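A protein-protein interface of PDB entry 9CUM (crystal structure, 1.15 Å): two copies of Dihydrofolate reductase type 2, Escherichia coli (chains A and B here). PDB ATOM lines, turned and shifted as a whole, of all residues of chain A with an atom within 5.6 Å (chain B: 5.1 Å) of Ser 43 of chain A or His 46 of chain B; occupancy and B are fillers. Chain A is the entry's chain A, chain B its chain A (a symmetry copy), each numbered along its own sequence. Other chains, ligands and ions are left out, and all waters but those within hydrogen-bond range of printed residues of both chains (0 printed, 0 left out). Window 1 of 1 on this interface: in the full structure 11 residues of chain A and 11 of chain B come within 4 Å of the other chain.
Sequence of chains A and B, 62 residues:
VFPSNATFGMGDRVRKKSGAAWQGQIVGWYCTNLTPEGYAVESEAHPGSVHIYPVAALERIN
NE2 of His 46 of chain B lies within hydrogen-bond range of OG of Ser 43 of chain A, at 2.7 Å.
O of Pro 47 of chain B is in hydrogen-bond range of N of Ala 21 of chain A (3.0 Å).
The side-chain hydroxyl of Ser 43 of chain B sits at hydrogen-bond distance from a ring nitrogen (NE2) of His 46 of chain A.
OE2 of Glu 44 of chain A sits close to OE1 of Gln 23 of chain A, 2.9 Å away.
The backbone NH of Ser 43 of chain B sits at hydrogen-bond distance from the backbone carbonyl oxygen of Ser 49 of chain B (2.9 Å).
The side-chain hydroxyl (OG) of Ser 43 of chain B is in hydrogen-bond range of the backbone NH (N) of Ala 45 of chain B (2.9 Å).
The backbone NH of Ser 43 of chain A sits at hydrogen-bond distance from the backbone carbonyl oxygen of Ser 49 of chain A (2.9 Å).
OG of Ser 43 of chain A sits at hydrogen-bond distance from N of His 46 of chain A (2.9 Å).
The backbone carbonyl oxygen of Val 41 of chain A lies within hydrogen-bond range of the indole nitrogen of Trp 22 of chain A, 2.9 Å away.
Ala 20 of chain A touches Pro 47 of chain B (CA to O, 3.7 Å).
Ala 20 of chain A touches Gly 48 of chain B (CB to O, 3.5 Å).
N of Ser 49 of chain B touches CB of Ala 20 of chain A, at 3.8 Å.
Ala 21 of chain A touches Ser 49 of chain B (O to CB, 3.6 Å).
Trp 22 of chain A touches His 46 of chain B (CE3 to CD2, 3.7 Å).
CE1 of His 46 of chain B touches N of Gln 23 of chain A, at 3.5 Å.
Ala 45 of chain B touches Ala 45 of chain A (CB to CB, 3.5 Å).
His 46 of chain B touches Ala 45 of chain A.
His 46 of chain A touches Ala 45 of chain B (NE2 to CB, 3.9 Å).
His 46 of chain B touches His 46 of chain A.
Of chain A, only Ala 21, Trp 22, Gln 23, Ser 43, Ala 45 and His 46 come within 4 Å of His 46 of chain B.
Printed residues of chain B within 4 Å of Trp 22 of chain A: His 46 (3.7 Å) and Ser 49 (3.7 Å).
Of the printed residues of chain B, Ala 21 of chain A touches His 46 (3.3 Å), Pro 47 (3.0 Å) and Ser 49 (3.6 Å).
Printed residues of chain B within 4 Å of Ala 20 of chain A: Pro 47, Gly 48 and Ser 49.
Of the printed residues of chain B, Ala 45 of chain A touches Ala 45 and His 46.
The nearest printed residue of chain B that does not touch Ser 43 of chain A is Ala 45 of chain B (6.0 Å).
Of the 8 printed residues of chain B, 6 touch a printed residue of chain A.
Hydrophobic or aromatic side chains of chain B within 4 Å of the printed part of chain A: Ala 45 and His 46.
Along chain B the printed residues that touch a printed residue of chain A span positions 43 to 49.
Hydrophobic or aromatic side chains of chain A within 4 Å of the printed part of chain B: Ala 20, Ala 21, Trp 22, Ala 45 and His 46.
Among the printed residues, no Asp or Glu carboxylate lies within 4 Å of a Lys or Arg side-chain nitrogen of the other chain.
Ser 43 of chain A touches His 46 of chain B, and with the chains exchanged His 46 of chain A touches Ser 43 of chain B.
Ala 45 of chain A touches its own counterpart, Ala 45 of chain B.
Ala 45 of chain A touches His 46 of chain B, and with the chains exchanged His 46 of chain A touches Ala 45 of chain B.
His 46 of chain A touches its own counterpart, His 46 of chain B.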
ATOM      1  N   ALA A  20     -27.679 -15.015  27.032  1.00  0.00           N
ATOM      2  CA  ALA A  20     -27.112 -14.487  25.806  1.00  0.00           C
ATOM      3  C   ALA A  20     -28.223 -13.840  24.995  1.00  0.00           C
ATOM      4  O   ALA A  20     -29.322 -14.377  24.827  1.00  0.00           O
ATOM      5  CB  ALA A  20     -26.461 -15.628  25.042  1.00  0.00           C
ATOM      6  N   ALA A  21     -27.932 -12.671  24.422  1.00  0.00           N
ATOM      7  CA  ALA A  21     -28.938 -11.885  23.752  1.00  0.00           C
ATOM      8  C   ALA A  21     -29.159 -12.346  22.326  1.00  0.00           C
ATOM      9  O   ALA A  21     -28.285 -12.883  21.652  1.00  0.00           O
ATOM     10  CB  ALA A  21     -28.545 -10.422  23.762  1.00  0.00           C
ATOM     11  N   TRP A  22     -30.366 -12.088  21.833  1.00  0.00           N
ATOM     12  CA  TRP A  22     -30.698 -12.300  20.431  1.00  0.00           C
ATOM     13  C   TRP A  22     -31.958 -11.493  20.142  1.00  0.00           C
ATOM     14  O   TRP A  22     -32.849 -11.439  20.975  1.00  0.00           O
ATOM     15  CB  TRP A  22     -30.958 -13.767  20.106  1.00  0.00           C
ATOM     16  CG  TRP A  22     -30.869 -14.061  18.642  1.00  0.00           C
ATOM     17  CD1 TRP A  22     -31.889 -14.304  17.774  1.00  0.00           C
ATOM     18  CD2 TRP A  22     -29.663 -14.133  17.883  1.00  0.00           C
ATOM     19  NE1 TRP A  22     -31.393 -14.529  16.513  1.00  0.00           N
ATOM     20  CE2 TRP A  22     -30.020 -14.446  16.568  1.00  0.00           C
ATOM     21  CE3 TRP A  22     -28.312 -14.001  18.206  1.00  0.00           C
ATOM     22  CZ2 TRP A  22     -29.088 -14.639  15.560  1.00  0.00           C
ATOM     23  CZ3 TRP A  22     -27.389 -14.197  17.208  1.00  0.00           C
ATOM     24  CH2 TRP A  22     -27.777 -14.507  15.913  1.00  0.00           C
ATOM     25  N   GLN A  23     -32.038 -10.856  18.978  1.00  0.00           N
ATOM     26  CA  GLN A  23     -33.203 -10.038  18.662  1.00  0.00           C
ATOM     27  C   GLN A  23     -33.331  -9.948  17.170  1.00  0.00           C
ATOM     28  O   GLN A  23     -32.337  -9.678  16.479  1.00  0.00           O
ATOM     29  CB  GLN A  23     -33.033  -8.659  19.302  1.00  0.00           C
ATOM     30  CG  GLN A  23     -34.261  -7.782  19.203  1.00  0.00           C
ATOM     31  CD  GLN A  23     -34.172  -6.566  20.074  1.00  0.00           C
ATOM     32  OE1 GLN A  23     -34.188  -5.431  19.581  1.00  0.00           O
ATOM     33  NE2 GLN A  23     -34.124  -6.797  21.345  1.00  0.00           N
ATOM     34  N   GLY A  24     -34.548 -10.097  16.656  1.00  0.00           N
ATOM     35  CA  GLY A  24     -34.806  -9.977  15.241  1.00  0.00           C
ATOM     36  C   GLY A  24     -36.130 -10.601  14.889  1.00  0.00           C
ATOM     37  O   GLY A  24     -37.002 -10.740  15.720  1.00  0.00           O
ATOM     38  N   GLN A  25     -36.294 -11.002  13.627  1.00  0.00           N
ATOM     39  CA  GLN A  25     -37.556 -11.476  13.135  1.00  0.00           C
ATOM     40  C   GLN A  25     -37.641 -12.976  13.084  1.00  0.00           C
ATOM     41  O   GLN A  25     -36.684 -13.682  12.741  1.00  0.00           O
ATOM     42  CB  GLN A  25     -37.827 -10.919  11.746  1.00  0.00           C
ATOM     43  CG  GLN A  25     -38.184  -9.421  11.753  1.00  0.00           C
ATOM     44  CD  GLN A  25     -38.486  -8.957  10.355  1.00  0.00           C
ATOM     45  OE1 GLN A  25     -39.353  -9.505   9.691  1.00  0.00           O
ATOM     46  NE2 GLN A  25     -37.629  -8.112   9.816  1.00  0.00           N
ATOM     47  N   VAL A  41     -34.927 -17.348  14.341  1.00  0.00           N
ATOM     48  CA  VAL A  41     -34.937 -15.908  14.448  1.00  0.00           C
ATOM     49  C   VAL A  41     -33.715 -15.365  13.736  1.00  0.00           C
ATOM     50  O   VAL A  41     -32.579 -15.699  14.123  1.00  0.00           O
ATOM     51  CB  VAL A  41     -34.936 -15.463  15.922  1.00  0.00           C
ATOM     52  CG1 VAL A  41     -35.016 -13.942  16.006  1.00  0.00           C
ATOM     53  CG2 VAL A  41     -36.060 -16.119  16.706  1.00  0.00           C
ATOM     54  N   GLU A  42     -33.904 -14.519  12.749  1.00  0.00           N
ATOM     55  CA  GLU A  42     -32.802 -13.863  12.064  1.00  0.00           C
ATOM     56  C   GLU A  42     -32.437 -12.595  12.817  1.00  0.00           C
ATOM     57  O   GLU A  42     -33.305 -11.738  13.045  1.00  0.00           O
ATOM     58  CB  GLU A  42     -33.162 -13.522  10.621  1.00  0.00           C
ATOM     59  CG  GLU A  42     -31.997 -12.923   9.855  1.00  0.00           C
ATOM     60  CD  GLU A  42     -32.282 -12.623   8.406  1.00  0.00           C
ATOM     61  OE1 GLU A  42     -33.457 -12.687   7.978  1.00  0.00           O
ATOM     62  OE2 GLU A  42     -31.315 -12.294   7.681  1.00  0.00           O
ATOM     63  N   SER A  43     -31.174 -12.437  13.192  1.00  0.00           N
ATOM     64  CA  SER A  43     -30.735 -11.229  13.874  1.00  0.00           C
ATOM     65  C   SER A  43     -31.024  -9.993  13.033  1.00  0.00           C
ATOM     66  O   SER A  43     -30.728  -9.963  11.834  1.00  0.00           O
ATOM     67  CB  SER A  43     -29.258 -11.291  14.138  1.00  0.00           C
ATOM     68  OG  SER A  43     -28.788 -10.049  14.636  1.00  0.00           O
ATOM     69  N   GLU A  44     -31.539  -8.963  13.695  1.00  0.00           N
ATOM     70  CA  GLU A  44     -31.696  -7.659  13.077  1.00  0.00           C
ATOM     71  C   GLU A  44     -30.398  -6.880  13.053  1.00  0.00           C
ATOM     72  O   GLU A  44     -30.315  -5.877  12.364  1.00  0.00           O
ATOM     73  CB  GLU A  44     -32.837  -6.885  13.704  1.00  0.00           C
ATOM     74  CG  GLU A  44     -32.571  -6.469  15.125  1.00  0.00           C
ATOM     75  CD  GLU A  44     -33.753  -5.911  15.857  1.00  0.00           C
ATOM     76  OE1 GLU A  44     -34.889  -6.313  15.574  1.00  0.00           O
ATOM     77  OE2 GLU A  44     -33.540  -5.112  16.814  1.00  0.00           O
ATOM     78  N   ALA A  45     -29.411  -7.286  13.838  1.00  0.00           N
ATOM     79  CA  ALA A  45     -28.110  -6.635  13.877  1.00  0.00           C
ATOM     80  C   ALA A  45     -27.117  -7.276  12.920  1.00  0.00           C
ATOM     81  O   ALA A  45     -26.244  -6.585  12.407  1.00  0.00           O
ATOM     82  CB  ALA A  45     -27.553  -6.682  15.284  1.00  0.00           C
ATOM     83  N   HIS A  46     -27.232  -8.583  12.721  1.00  0.00           N
ATOM     84  CA  HIS A  46     -26.289  -9.357  11.924  1.00  0.00           C
ATOM     85  C   HIS A  46     -27.087 -10.055  10.820  1.00  0.00           C
ATOM     86  O   HIS A  46     -27.453 -11.227  10.962  1.00  0.00           O
ATOM     87  CB  HIS A  46     -25.555 -10.381  12.779  1.00  0.00           C
ATOM     88  CG  HIS A  46     -24.767  -9.830  13.914  1.00  0.00           C
ATOM     89  ND1 HIS A  46     -23.829  -8.841  13.796  1.00  0.00           N
ATOM     90  CD2 HIS A  46     -24.711 -10.209  15.207  1.00  0.00           C
ATOM     91  CE1 HIS A  46     -23.277  -8.658  15.002  1.00  0.00           C
ATOM     92  NE2 HIS A  46     -23.772  -9.484  15.884  1.00  0.00           N
ATOM     93  N   PRO A  47     -27.378  -9.356   9.720  1.00  0.00           N
ATOM     94  CA  PRO A  47     -28.199  -9.948   8.674  1.00  0.00           C
ATOM     95  C   PRO A  47     -27.670 -11.296   8.243  1.00  0.00           C
ATOM     96  O   PRO A  47     -26.461 -11.486   8.043  1.00  0.00           O
ATOM     97  CB  PRO A  47     -28.156  -8.912   7.553  1.00  0.00           C
ATOM     98  CG  PRO A  47     -27.934  -7.619   8.263  1.00  0.00           C
ATOM     99  CD  PRO A  47     -27.006  -7.966   9.395  1.00  0.00           C
ATOM    100  N   GLY A  48     -28.601 -12.233   8.019  1.00  0.00           N
ATOM    101  CA  GLY A  48     -28.266 -13.572   7.592  1.00  0.00           C
ATOM    102  C   GLY A  48     -28.004 -14.546   8.717  1.00  0.00           C
ATOM    103  O   GLY A  48     -28.068 -15.762   8.483  1.00  0.00           O
ATOM    104  N   SER A  49     -27.668 -14.054   9.913  1.00  0.00           N
ATOM    105  CA  SER A  49     -27.385 -14.864  11.080  1.00  0.00           C
ATOM    106  C   SER A  49     -28.691 -15.319  11.716  1.00  0.00           C
ATOM    107  O   SER A  49     -29.488 -14.451  12.072  1.00  0.00           O
ATOM    108  CB  SER A  49     -26.590 -14.010  12.061  1.00  0.00           C
ATOM    109  OG  SER A  49     -26.125 -14.833  13.097  1.00  0.00           O
ATOM    110  N   VAL A  50     -28.888 -16.616  11.889  1.00  0.00           N
ATOM    111  CA  VAL A  50     -30.132 -17.171  12.417  1.00  0.00           C
ATOM    112  C   VAL A  50     -29.817 -18.068  13.597  1.00  0.00           C
ATOM    113  O   VAL A  50     -28.917 -18.900  13.511  1.00  0.00           O
ATOM    114  CB  VAL A  50     -30.875 -17.962  11.324  1.00  0.00           C
ATOM    115  CG1 VAL A  50     -32.166 -18.567  11.840  1.00  0.00           C
ATOM    116  CG2 VAL A  50     -31.158 -17.092  10.122  1.00  0.00           C
ATOM    117  N   GLU B  42     -17.514 -12.963  20.442  1.00  0.00           N
ATOM    118  CA  GLU B  42     -18.719 -12.518  21.123  1.00  0.00           C
ATOM    119  C   GLU B  42     -19.312 -11.344  20.363  1.00  0.00           C
ATOM    120  O   GLU B  42     -18.617 -10.343  20.129  1.00  0.00           O
ATOM    121  CB  GLU B  42     -18.428 -12.107  22.565  1.00  0.00           C
ATOM    122  CG  GLU B  42     -19.685 -11.729  23.328  1.00  0.00           C
ATOM    123  CD  GLU B  42     -19.462 -11.372  24.774  1.00  0.00           C
ATOM    124  OE1 GLU B  42     -18.295 -11.215  25.202  1.00  0.00           O
ATOM    125  OE2 GLU B  42     -20.473 -11.224  25.498  1.00  0.00           O
ATOM    126  N   SER B  43     -20.582 -11.426  19.988  1.00  0.00           N
ATOM    127  CA  SER B  43     -21.236 -10.324  19.298  1.00  0.00           C
ATOM    128  C   SER B  43     -21.182  -9.051  20.131  1.00  0.00           C
ATOM    129  O   SER B  43     -21.479  -9.068  21.330  1.00  0.00           O
ATOM    130  CB  SER B  43     -22.676 -10.661  19.035  1.00  0.00           C
ATOM    131  OG  SER B  43     -23.368  -9.530  18.530  1.00  0.00           O
ATOM    132  N   GLU B  44     -20.867  -7.947  19.462  1.00  0.00           N
ATOM    133  CA  GLU B  44     -20.954  -6.633  20.071  1.00  0.00           C
ATOM    134  C   GLU B  44     -22.373  -6.108  20.091  1.00  0.00           C
ATOM    135  O   GLU B  44     -22.642  -5.133  20.774  1.00  0.00           O
ATOM    136  CB  GLU B  44     -19.975  -5.665  19.439  1.00  0.00           C
ATOM    137  CG  GLU B  44     -20.313  -5.315  18.016  1.00  0.00           C
ATOM    138  CD  GLU B  44     -19.254  -4.553  17.279  1.00  0.00           C
ATOM    139  OE1 GLU B  44     -18.064  -4.735  17.564  1.00  0.00           O
ATOM    140  OE2 GLU B  44     -19.611  -3.813  16.317  1.00  0.00           O
ATOM    141  N   ALA B  45     -23.267  -6.694  19.310  1.00  0.00           N
ATOM    142  CA  ALA B  45     -24.666  -6.296  19.267  1.00  0.00           C
ATOM    143  C   ALA B  45     -25.525  -7.104  20.228  1.00  0.00           C
ATOM    144  O   ALA B  45     -26.511  -6.583  20.738  1.00  0.00           O
ATOM    145  CB  ALA B  45     -25.204  -6.454  17.860  1.00  0.00           C
ATOM    146  N   HIS B  46     -25.170  -8.365  20.436  1.00  0.00           N
ATOM    147  CA  HIS B  46     -25.954  -9.296  21.239  1.00  0.00           C
ATOM    148  C   HIS B  46     -25.041  -9.826  22.347  1.00  0.00           C
ATOM    149  O   HIS B  46     -24.463 -10.911  22.212  1.00  0.00           O
ATOM    150  CB  HIS B  46     -26.485 -10.443  20.391  1.00  0.00           C
ATOM    151  CG  HIS B  46     -27.360 -10.055  19.252  1.00  0.00           C
ATOM    152  ND1 HIS B  46     -28.466  -9.256  19.365  1.00  0.00           N
ATOM    153  CD2 HIS B  46     -27.344 -10.446  17.963  1.00  0.00           C
ATOM    154  CE1 HIS B  46     -29.041  -9.186  18.158  1.00  0.00           C
ATOM    155  NE2 HIS B  46     -28.401  -9.911  17.281  1.00  0.00           N
ATOM    156  N   PRO B  47     -24.884  -9.079  23.442  1.00  0.00           N
ATOM    157  CA  PRO B  47     -23.969  -9.502  24.492  1.00  0.00           C
ATOM    158  C   PRO B  47     -24.239 -10.921  24.931  1.00  0.00           C
ATOM    159  O   PRO B  47     -25.393 -11.331  25.133  1.00  0.00           O
ATOM    160  CB  PRO B  47     -24.204  -8.484  25.605  1.00  0.00           C
ATOM    161  CG  PRO B  47     -24.660  -7.259  24.888  1.00  0.00           C
ATOM    162  CD  PRO B  47     -25.508  -7.779  23.758  1.00  0.00           C
ATOM    163  N   GLY B  48     -23.151 -11.668  25.161  1.00  0.00           N
ATOM    164  CA  GLY B  48     -23.233 -13.043  25.597  1.00  0.00           C
ATOM    165  C   GLY B  48     -23.310 -14.057  24.478  1.00  0.00           C
ATOM    166  O   GLY B  48     -23.022 -15.238  24.720  1.00  0.00           O
ATOM    167  N   SER B  49     -23.729 -13.642  23.279  1.00  0.00           N
ATOM    168  CA  SER B  49     -23.857 -14.499  22.118  1.00  0.00           C
ATOM    169  C   SER B  49     -22.489 -14.708  21.484  1.00  0.00           C
ATOM    170  O   SER B  49     -21.867 -13.710  21.121  1.00  0.00           O
ATOM    171  CB  SER B  49     -24.796 -13.813  21.132  1.00  0.00           C
ATOM    172  OG  SER B  49     -25.099 -14.714  20.101  1.00  0.00           O
